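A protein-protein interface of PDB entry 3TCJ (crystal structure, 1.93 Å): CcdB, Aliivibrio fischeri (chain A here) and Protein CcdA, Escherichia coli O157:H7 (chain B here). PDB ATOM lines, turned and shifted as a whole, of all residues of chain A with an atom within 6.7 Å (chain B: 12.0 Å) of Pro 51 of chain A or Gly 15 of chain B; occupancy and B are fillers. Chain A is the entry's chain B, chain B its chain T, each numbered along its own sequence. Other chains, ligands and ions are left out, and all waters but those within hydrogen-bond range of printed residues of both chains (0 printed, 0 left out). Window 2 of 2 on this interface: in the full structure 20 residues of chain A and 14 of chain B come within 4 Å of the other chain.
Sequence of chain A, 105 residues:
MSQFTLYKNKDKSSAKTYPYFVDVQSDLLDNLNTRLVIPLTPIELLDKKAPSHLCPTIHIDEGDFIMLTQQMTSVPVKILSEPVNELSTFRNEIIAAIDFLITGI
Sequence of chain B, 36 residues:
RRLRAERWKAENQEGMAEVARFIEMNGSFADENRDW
CG2 of Val 19 of chain B touches CB of Ala 50 of chain A, at 3.4 Å. Gly 15 of chain B touches Pro 51 of chain A. Gln 70 of chain A touches Val 19 of chain B (NE2 to CG1, 3.2 Å). Ile 23 of chain B touches Gln 70 of chain A (CD1 to NE2, 3.6 Å). Trp 8 of chain B touches Phe 100 of chain A (CZ2 to CZ, 3.5 Å).
O of Trp 8 of chain B lies close to OD1 of Asn 12 of chain B.
Of the 19 printed residues of chain B, 4 touch a printed residue of chain A.
Of chain B, only Gly 15 comes within 4 Å of Pro 51 of chain A. Of the printed residues of chain A, Gly 15 of chain B touches Pro 51 (3.9 Å). No residue of chain B comes within 4 Å of Lys 49 of chain A. Ala 50 of chain A touches just one residue of chain B: Val 19 (3.4 Å). No residue of chain B comes within 4 Å of Ser 52 of chain A. No residue of chain B comes within 4 Å of His 53 of chain A. No residue of chain B comes within 4 Å of Leu 54 of chain A. No residue of chain B comes within 4 Å of Cys 55 of chain A. Pro 56 of chain A touches none of the printed residues of chain B. Of the printed residues of chain A, Ile 23 of chain B touches Gln 70. Printed residues of chain A within 4 Å of Val 19 of chain B: Ala 50 (3.4 Å) and Gln 70 (3.2 Å). Printed residues of chain B within 4 Å of Phe 100 of chain A: Trp 8 (3.5 Å). Printed residues of chain A within 4 Å of Trp 8 of chain B: Phe 100 (3.5 Å). Glu 18 of chain B touches none of the printed residues of chain A. Met 16 of chain B touches none of the printed residues of chain A. The nearest residue of chain B that does not touch Pro 51 of chain A is Asn 12 of chain B (4.1 Å). The nearest residue of chain A that does not touch Gly 15 of chain B is Lys 49 of chain A (4.1 Å). The nearest printed residue of chain B that does not touch Gln 70 of chain A is Ala 20 of chain B (5.0 Å).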
ATOM      1  N   LYS A  49      -8.604 -26.624 -29.406  1.00  0.00           N
ATOM      2  CA  LYS A  49      -7.243 -26.120 -29.550  1.00  0.00           C
ATOM      3  C   LYS A  49      -6.864 -25.190 -28.401  1.00  0.00           C
ATOM      4  O   LYS A  49      -7.093 -23.983 -28.464  1.00  0.00           O
ATOM      5  CB  LYS A  49      -7.077 -25.394 -30.888  1.00  0.00           C
ATOM      6  N   ALA A  50      -6.285 -25.764 -27.351  1.00  0.00           N
ATOM      7  CA  ALA A  50      -5.820 -24.987 -26.210  1.00  0.00           C
ATOM      8  C   ALA A  50      -4.501 -24.296 -26.543  1.00  0.00           C
ATOM      9  O   ALA A  50      -3.800 -24.712 -27.465  1.00  0.00           O
ATOM     10  CB  ALA A  50      -5.643 -25.895 -24.992  1.00  0.00           C
ATOM     11  N   PRO A  51      -4.162 -23.233 -25.795  1.00  0.00           N
ATOM     12  CA  PRO A  51      -2.886 -22.535 -25.992  1.00  0.00           C
ATOM     13  C   PRO A  51      -1.716 -23.514 -25.975  1.00  0.00           C
ATOM     14  O   PRO A  51      -1.394 -24.077 -24.928  1.00  0.00           O
ATOM     15  CB  PRO A  51      -2.816 -21.596 -24.786  1.00  0.00           C
ATOM     16  CG  PRO A  51      -4.238 -21.338 -24.434  1.00  0.00           C
ATOM     17  CD  PRO A  51      -4.971 -22.617 -24.730  1.00  0.00           C
ATOM     18  N   SER A  52      -1.091 -23.709 -27.131  1.00  0.00           N
ATOM     19  CA  SER A  52      -0.032 -24.701 -27.287  1.00  0.00           C
ATOM     20  C   SER A  52       1.108 -24.549 -26.281  1.00  0.00           C
ATOM     21  O   SER A  52       1.648 -25.543 -25.797  1.00  0.00           O
ATOM     22  N   HIS A  53       1.476 -23.309 -25.975  1.00  0.00           N
ATOM     23  CA  HIS A  53       2.588 -23.047 -25.062  1.00  0.00           C
ATOM     24  C   HIS A  53       2.286 -23.506 -23.641  1.00  0.00           C
ATOM     25  O   HIS A  53       3.196 -23.835 -22.879  1.00  0.00           O
ATOM     26  CB  HIS A  53       2.955 -21.562 -25.065  1.00  0.00           C
ATOM     27  CG  HIS A  53       3.710 -21.132 -26.282  1.00  0.00           C
ATOM     28  ND1 HIS A  53       5.050 -20.807 -26.253  1.00  0.00           N
ATOM     29  CD2 HIS A  53       3.316 -20.985 -27.569  1.00  0.00           C
ATOM     30  CE1 HIS A  53       5.446 -20.472 -27.468  1.00  0.00           C
ATOM     31  NE2 HIS A  53       4.413 -20.573 -28.285  1.00  0.00           N
ATOM     32  N   LEU A  54       1.005 -23.527 -23.288  1.00  0.00           N
ATOM     33  CA  LEU A  54       0.598 -23.894 -21.940  1.00  0.00           C
ATOM     34  C   LEU A  54       0.161 -25.354 -21.859  1.00  0.00           C
ATOM     35  O   LEU A  54       0.280 -25.988 -20.811  1.00  0.00           O
ATOM     36  CB  LEU A  54      -0.531 -22.980 -21.461  1.00  0.00           C
ATOM     37  CG  LEU A  54      -1.073 -23.252 -20.057  1.00  0.00           C
ATOM     38  CD1 LEU A  54       0.031 -23.115 -19.015  1.00  0.00           C
ATOM     39  CD2 LEU A  54      -2.233 -22.318 -19.745  1.00  0.00           C
ATOM     40  N   CYS A  55      -0.339 -25.881 -22.971  1.00  0.00           N
ATOM     41  CA  CYS A  55      -0.844 -27.248 -23.010  1.00  0.00           C
ATOM     42  C   CYS A  55      -0.218 -28.046 -24.148  1.00  0.00           C
ATOM     43  O   CYS A  55      -0.793 -28.142 -25.230  1.00  0.00           O
ATOM     44  CB  CYS A  55      -2.366 -27.245 -23.161  1.00  0.00           C
ATOM     45  SG  CYS A  55      -3.232 -26.200 -21.968  1.00  0.00           S
ATOM     46  N   PRO A  56       0.967 -28.626 -23.902  1.00  0.00           N
ATOM     47  CA  PRO A  56       1.702 -29.396 -24.913  1.00  0.00           C
ATOM     48  C   PRO A  56       0.933 -30.631 -25.369  1.00  0.00           C
ATOM     49  O   PRO A  56       0.204 -31.235 -24.581  1.00  0.00           O
ATOM     50  CB  PRO A  56       2.972 -29.832 -24.172  1.00  0.00           C
ATOM     51  CG  PRO A  56       3.095 -28.901 -23.014  1.00  0.00           C
ATOM     52  CD  PRO A  56       1.693 -28.557 -22.623  1.00  0.00           C
ATOM     53  N   GLN A  70      -2.127 -26.489 -16.357  1.00  0.00           N
ATOM     54  CA  GLN A  70      -2.879 -25.646 -15.434  1.00  0.00           C
ATOM     55  C   GLN A  70      -3.568 -26.471 -14.345  1.00  0.00           C
ATOM     56  O   GLN A  70      -4.103 -25.921 -13.384  1.00  0.00           O
ATOM     57  CB  GLN A  70      -3.909 -24.805 -16.196  1.00  0.00           C
ATOM     58  CG  GLN A  70      -5.074 -25.602 -16.757  1.00  0.00           C
ATOM     59  CD  GLN A  70      -5.799 -24.870 -17.871  1.00  0.00           C
ATOM     60  OE1 GLN A  70      -5.231 -24.615 -18.935  1.00  0.00           O
ATOM     61  NE2 GLN A  70      -7.062 -24.532 -17.636  1.00  0.00           N
ATOM     62  N   PHE A 100       6.450 -21.594 -18.598  1.00  0.00           N
ATOM     63  CA  PHE A 100       5.460 -20.659 -19.121  1.00  0.00           C
ATOM     64  C   PHE A 100       4.397 -20.331 -18.076  1.00  0.00           C
ATOM     65  O   PHE A 100       4.004 -19.175 -17.914  1.00  0.00           O
ATOM     66  CB  PHE A 100       4.803 -21.236 -20.374  1.00  0.00           C
ATOM     67  CG  PHE A 100       3.988 -20.239 -21.143  1.00  0.00           C
ATOM     68  CD1 PHE A 100       4.603 -19.323 -21.980  1.00  0.00           C
ATOM     69  CD2 PHE A 100       2.608 -20.218 -21.032  1.00  0.00           C
ATOM     70  CE1 PHE A 100       3.854 -18.401 -22.692  1.00  0.00           C
ATOM     71  CE2 PHE A 100       1.854 -19.301 -21.740  1.00  0.00           C
ATOM     72  CZ  PHE A 100       2.478 -18.392 -22.571  1.00  0.00           C
ATOM     73  N   ALA B   5       1.454  -7.634 -23.740  1.00  0.00           N
ATOM     74  CA  ALA B   5       0.945  -8.720 -22.910  1.00  0.00           C
ATOM     75  C   ALA B   5      -0.579  -8.781 -22.943  1.00  0.00           C
ATOM     76  O   ALA B   5      -1.168  -9.863 -22.899  1.00  0.00           O
ATOM     77  CB  ALA B   5       1.438  -8.570 -21.480  1.00  0.00           C
ATOM     78  N   ARG B   7      -2.528  -7.881 -25.456  1.00  0.00           N
ATOM     79  CA  ARG B   7      -2.960  -8.427 -26.737  1.00  0.00           C
ATOM     80  C   ARG B   7      -2.802  -9.943 -26.763  1.00  0.00           C
ATOM     81  O   ARG B   7      -3.633 -10.649 -27.333  1.00  0.00           O
ATOM     82  CB  ARG B   7      -2.209  -7.787 -27.906  1.00  0.00           C
ATOM     83  CG  ARG B   7      -2.659  -8.325 -29.255  1.00  0.00           C
ATOM     84  CD  ARG B   7      -2.385  -7.353 -30.390  1.00  0.00           C
ATOM     85  NE  ARG B   7      -3.347  -7.527 -31.476  1.00  0.00           N
ATOM     86  CZ  ARG B   7      -3.179  -8.352 -32.506  1.00  0.00           C
ATOM     87  NH1 ARG B   7      -2.076  -9.084 -32.605  1.00  0.00           N
ATOM     88  NH2 ARG B   7      -4.115  -8.443 -33.441  1.00  0.00           N
ATOM     89  N   TRP B   8      -1.737 -10.443 -26.145  1.00  0.00           N
ATOM     90  CA  TRP B   8      -1.552 -11.885 -26.041  1.00  0.00           C
ATOM     91  C   TRP B   8      -2.728 -12.497 -25.290  1.00  0.00           C
ATOM     92  O   TRP B   8      -3.292 -13.502 -25.718  1.00  0.00           O
ATOM     93  CB  TRP B   8      -0.237 -12.235 -25.341  1.00  0.00           C
ATOM     94  CG  TRP B   8       0.051 -13.707 -25.363  1.00  0.00           C
ATOM     95  CD1 TRP B   8       0.886 -14.368 -26.219  1.00  0.00           C
ATOM     96  CD2 TRP B   8      -0.517 -14.707 -24.506  1.00  0.00           C
ATOM     97  NE1 TRP B   8       0.880 -15.712 -25.942  1.00  0.00           N
ATOM     98  CE2 TRP B   8       0.027 -15.948 -24.895  1.00  0.00           C
ATOM     99  CE3 TRP B   8      -1.428 -14.673 -23.445  1.00  0.00           C
ATOM    100  CZ2 TRP B   8      -0.310 -17.142 -24.263  1.00  0.00           C
ATOM    101  CZ3 TRP B   8      -1.760 -15.859 -22.819  1.00  0.00           C
ATOM    102  CH2 TRP B   8      -1.203 -17.078 -23.229  1.00  0.00           C
ATOM    103  N   LYS B   9      -3.093 -11.883 -24.168  1.00  0.00           N
ATOM    104  CA  LYS B   9      -4.242 -12.334 -23.391  1.00  0.00           C
ATOM    105  C   LYS B   9      -5.494 -12.313 -24.254  1.00  0.00           C
ATOM    106  O   LYS B   9      -6.264 -13.271 -24.272  1.00  0.00           O
ATOM    107  CB  LYS B   9      -4.455 -11.442 -22.164  1.00  0.00           C
ATOM    108  CG  LYS B   9      -3.383 -11.557 -21.093  1.00  0.00           C
ATOM    109  CD  LYS B   9      -3.731 -10.700 -19.880  1.00  0.00           C
ATOM    110  CE  LYS B   9      -2.645 -10.772 -18.817  1.00  0.00           C
ATOM    111  NZ  LYS B   9      -2.942  -9.905 -17.641  1.00  0.00           N
ATOM    112  N   ALA B  10      -5.685 -11.208 -24.970  1.00  0.00           N
ATOM    113  CA  ALA B  10      -6.853 -11.031 -25.822  1.00  0.00           C
ATOM    114  C   ALA B  10      -6.936 -12.120 -26.884  1.00  0.00           C
ATOM    115  O   ALA B  10      -7.992 -12.711 -27.099  1.00  0.00           O
ATOM    116  CB  ALA B  10      -6.829  -9.653 -26.474  1.00  0.00           C
ATOM    117  N   GLU B  11      -5.811 -12.382 -27.543  1.00  0.00           N
ATOM    118  CA  GLU B  11      -5.757 -13.383 -28.601  1.00  0.00           C
ATOM    119  C   GLU B  11      -6.053 -14.784 -28.076  1.00  0.00           C
ATOM    120  O   GLU B  11      -6.729 -15.570 -28.732  1.00  0.00           O
ATOM    121  CB  GLU B  11      -4.386 -13.366 -29.285  1.00  0.00           C
ATOM    122  CG  GLU B  11      -4.103 -12.109 -30.088  1.00  0.00           C
ATOM    123  CD  GLU B  11      -4.927 -12.029 -31.360  1.00  0.00           C
ATOM    124  OE1 GLU B  11      -5.574 -13.037 -31.716  1.00  0.00           O
ATOM    125  OE2 GLU B  11      -4.925 -10.959 -32.002  1.00  0.00           O
ATOM    126  N   ASN B  12      -5.543 -15.088 -26.887  1.00  0.00           N
ATOM    127  CA  ASN B  12      -5.685 -16.423 -26.315  1.00  0.00           C
ATOM    128  C   ASN B  12      -6.901 -16.569 -25.401  1.00  0.00           C
ATOM    129  O   ASN B  12      -7.032 -17.566 -24.690  1.00  0.00           O
ATOM    130  CB  ASN B  12      -4.407 -16.817 -25.569  1.00  0.00           C
ATOM    131  CG  ASN B  12      -3.229 -17.031 -26.504  1.00  0.00           C
ATOM    132  OD1 ASN B  12      -2.393 -16.146 -26.682  1.00  0.00           O
ATOM    133  ND2 ASN B  12      -3.168 -18.207 -27.115  1.00  0.00           N
ATOM    134  N   GLN B  13      -7.787 -15.577 -25.423  1.00  0.00           N
ATOM    135  CA  GLN B  13      -8.981 -15.600 -24.582  1.00  0.00           C
ATOM    136  C   GLN B  13      -9.873 -16.806 -24.873  1.00  0.00           C
ATOM    137  O   GLN B  13     -10.256 -17.539 -23.961  1.00  0.00           O
ATOM    138  CB  GLN B  13      -9.789 -14.308 -24.745  1.00  0.00           C
ATOM    139  CG  GLN B  13      -9.309 -13.140 -23.897  1.00  0.00           C
ATOM    140  CD  GLN B  13     -10.205 -11.922 -24.037  1.00  0.00           C
ATOM    141  OE1 GLN B  13     -11.115 -11.904 -24.867  1.00  0.00           O
ATOM    142  NE2 GLN B  13      -9.953 -10.899 -23.227  1.00  0.00           N
ATOM    143  N   GLU B  14     -10.204 -17.003 -26.145  1.00  0.00           N
ATOM    144  CA  GLU B  14     -11.094 -18.090 -26.546  1.00  0.00           C
ATOM    145  C   GLU B  14     -10.486 -19.459 -26.257  1.00  0.00           C
ATOM    146  O   GLU B  14     -11.188 -20.387 -25.851  1.00  0.00           O
ATOM    147  CB  GLU B  14     -11.457 -17.975 -28.029  1.00  0.00           C
ATOM    148  N   GLY B  15      -9.180 -19.583 -26.470  1.00  0.00           N
ATOM    149  CA  GLY B  15      -8.483 -20.821 -26.180  1.00  0.00           C
ATOM    150  C   GLY B  15      -8.609 -21.181 -24.714  1.00  0.00           C
ATOM    151  O   GLY B  15      -8.895 -22.325 -24.366  1.00  0.00           O
ATOM    152  N   MET B  16      -8.400 -20.191 -23.852  1.00  0.00           N
ATOM    153  CA  MET B  16      -8.511 -20.390 -22.411  1.00  0.00           C
ATOM    154  C   MET B  16      -9.947 -20.682 -21.992  1.00  0.00           C
ATOM    155  O   MET B  16     -10.197 -21.591 -21.202  1.00  0.00           O
ATOM    156  CB  MET B  16      -7.989 -19.168 -21.657  1.00  0.00           C
ATOM    157  CG  MET B  16      -6.489 -18.977 -21.747  1.00  0.00           C
ATOM    158  SD  MET B  16      -5.912 -17.633 -20.696  1.00  0.00           S
ATOM    159  CE  MET B  16      -4.145 -17.753 -20.945  1.00  0.00           C
ATOM    160  N   ALA B  17     -10.886 -19.900 -22.519  1.00  0.00           N
ATOM    161  CA  ALA B  17     -12.298 -20.082 -22.201  1.00  0.00           C
ATOM    162  C   ALA B  17     -12.751 -21.504 -22.520  1.00  0.00           C
ATOM    163  O   ALA B  17     -13.418 -22.148 -21.710  1.00  0.00           O
ATOM    164  CB  ALA B  17     -13.150 -19.066 -22.951  1.00  0.00           C
ATOM    165  N   GLU B  18     -12.380 -21.989 -23.700  1.00  0.00           N
ATOM    166  CA  GLU B  18     -12.747 -23.337 -24.122  1.00  0.00           C
ATOM    167  C   GLU B  18     -12.241 -24.374 -23.123  1.00  0.00           C
ATOM    168  O   GLU B  18     -12.970 -25.294 -22.745  1.00  0.00           O
ATOM    169  CB  GLU B  18     -12.199 -23.636 -25.520  1.00  0.00           C
ATOM    170  N   VAL B  19     -10.993 -24.217 -22.697  1.00  0.00           N
ATOM    171  CA  VAL B  19     -10.393 -25.126 -21.727  1.00  0.00           C
ATOM    172  C   VAL B  19     -11.133 -25.073 -20.395  1.00  0.00           C
ATOM    173  O   VAL B  19     -11.421 -26.107 -19.793  1.00  0.00           O
ATOM    174  CB  VAL B  19      -8.909 -24.795 -21.488  1.00  0.00           C
ATOM    175  CG1 VAL B  19      -8.370 -25.592 -20.309  1.00  0.00           C
ATOM    176  CG2 VAL B  19      -8.098 -25.069 -22.744  1.00  0.00           C
ATOM    177  N   ALA B  20     -11.433 -23.859 -19.942  1.00  0.00           N
ATOM    178  CA  ALA B  20     -12.158 -23.661 -18.692  1.00  0.00           C
ATOM    179  C   ALA B  20     -13.516 -24.359 -18.723  1.00  0.00           C
ATOM    180  O   ALA B  20     -13.877 -25.067 -17.783  1.00  0.00           O
ATOM    181  CB  ALA B  20     -12.323 -22.176 -18.402  1.00  0.00           C
ATOM    182  N   ARG B  21     -14.264 -24.160 -19.803  1.00  0.00           N
ATOM    183  CA  ARG B  21     -15.559 -24.816 -19.958  1.00  0.00           C
ATOM    184  C   ARG B  21     -15.400 -26.331 -20.013  1.00  0.00           C
ATOM    185  O   ARG B  21     -16.281 -27.074 -19.580  1.00  0.00           O
ATOM    186  CB  ARG B  21     -16.281 -24.317 -21.212  1.00  0.00           C
ATOM    187  CG  ARG B  21     -16.858 -22.916 -21.086  1.00  0.00           C
ATOM    188  N   PHE B  22     -14.272 -26.784 -20.550  1.00  0.00           N
ATOM    189  CA  PHE B  22     -13.989 -28.211 -20.635  1.00  0.00           C
ATOM    190  C   PHE B  22     -13.802 -28.821 -19.250  1.00  0.00           C
ATOM    191  O   PHE B  22     -14.305 -29.907 -18.965  1.00  0.00           O
ATOM    192  CB  PHE B  22     -12.747 -28.466 -21.490  1.00  0.00           C
ATOM    193  CG  PHE B  22     -12.182 -29.847 -21.333  1.00  0.00           C
ATOM    194  CD1 PHE B  22     -12.765 -30.923 -21.976  1.00  0.00           C
ATOM    195  CD2 PHE B  22     -11.071 -30.069 -20.536  1.00  0.00           C
ATOM    196  CE1 PHE B  22     -12.250 -32.195 -21.829  1.00  0.00           C
ATOM    197  CE2 PHE B  22     -10.550 -31.339 -20.385  1.00  0.00           C
ATOM    198  CZ  PHE B  22     -11.141 -32.403 -21.032  1.00  0.00           C
ATOM    199  N   ILE B  23     -13.072 -28.113 -18.396  1.00  0.00           N
ATOM    200  CA  ILE B  23     -12.802 -28.581 -17.042  1.00  0.00           C
ATOM    201  C   ILE B  23     -14.051 -28.516 -16.162  1.00  0.00           C
ATOM    202  O   ILE B  23     -14.241 -29.345 -15.272  1.00  0.00           O
ATOM    203  CB  ILE B  23     -11.657 -27.775 -16.393  1.00  0.00           C
ATOM    204  CG1 ILE B  23     -10.353 -27.989 -17.166  1.00  0.00           C
ATOM    205  CG2 ILE B  23     -11.480 -28.169 -14.936  1.00  0.00           C
ATOM    206  CD1 ILE B  23      -9.155 -27.277 -16.564  1.00  0.00           C
ATOM    207  N   GLU B  24     -14.903 -27.530 -16.418  1.00  0.00           N
ATOM    208  CA  GLU B  24     -16.147 -27.388 -15.672  1.00  0.00           C
ATOM    209  C   GLU B  24     -17.118 -28.508 -16.023  1.00  0.00           C
ATOM    210  O   GLU B  24     -17.866 -28.988 -15.170  1.00  0.00           O
ATOM    211  CB  GLU B  24     -16.790 -26.028 -15.957  1.00  0.00           C
ATOM    212  CG  GLU B  24     -18.139 -25.827 -15.288  1.00  0.00           C
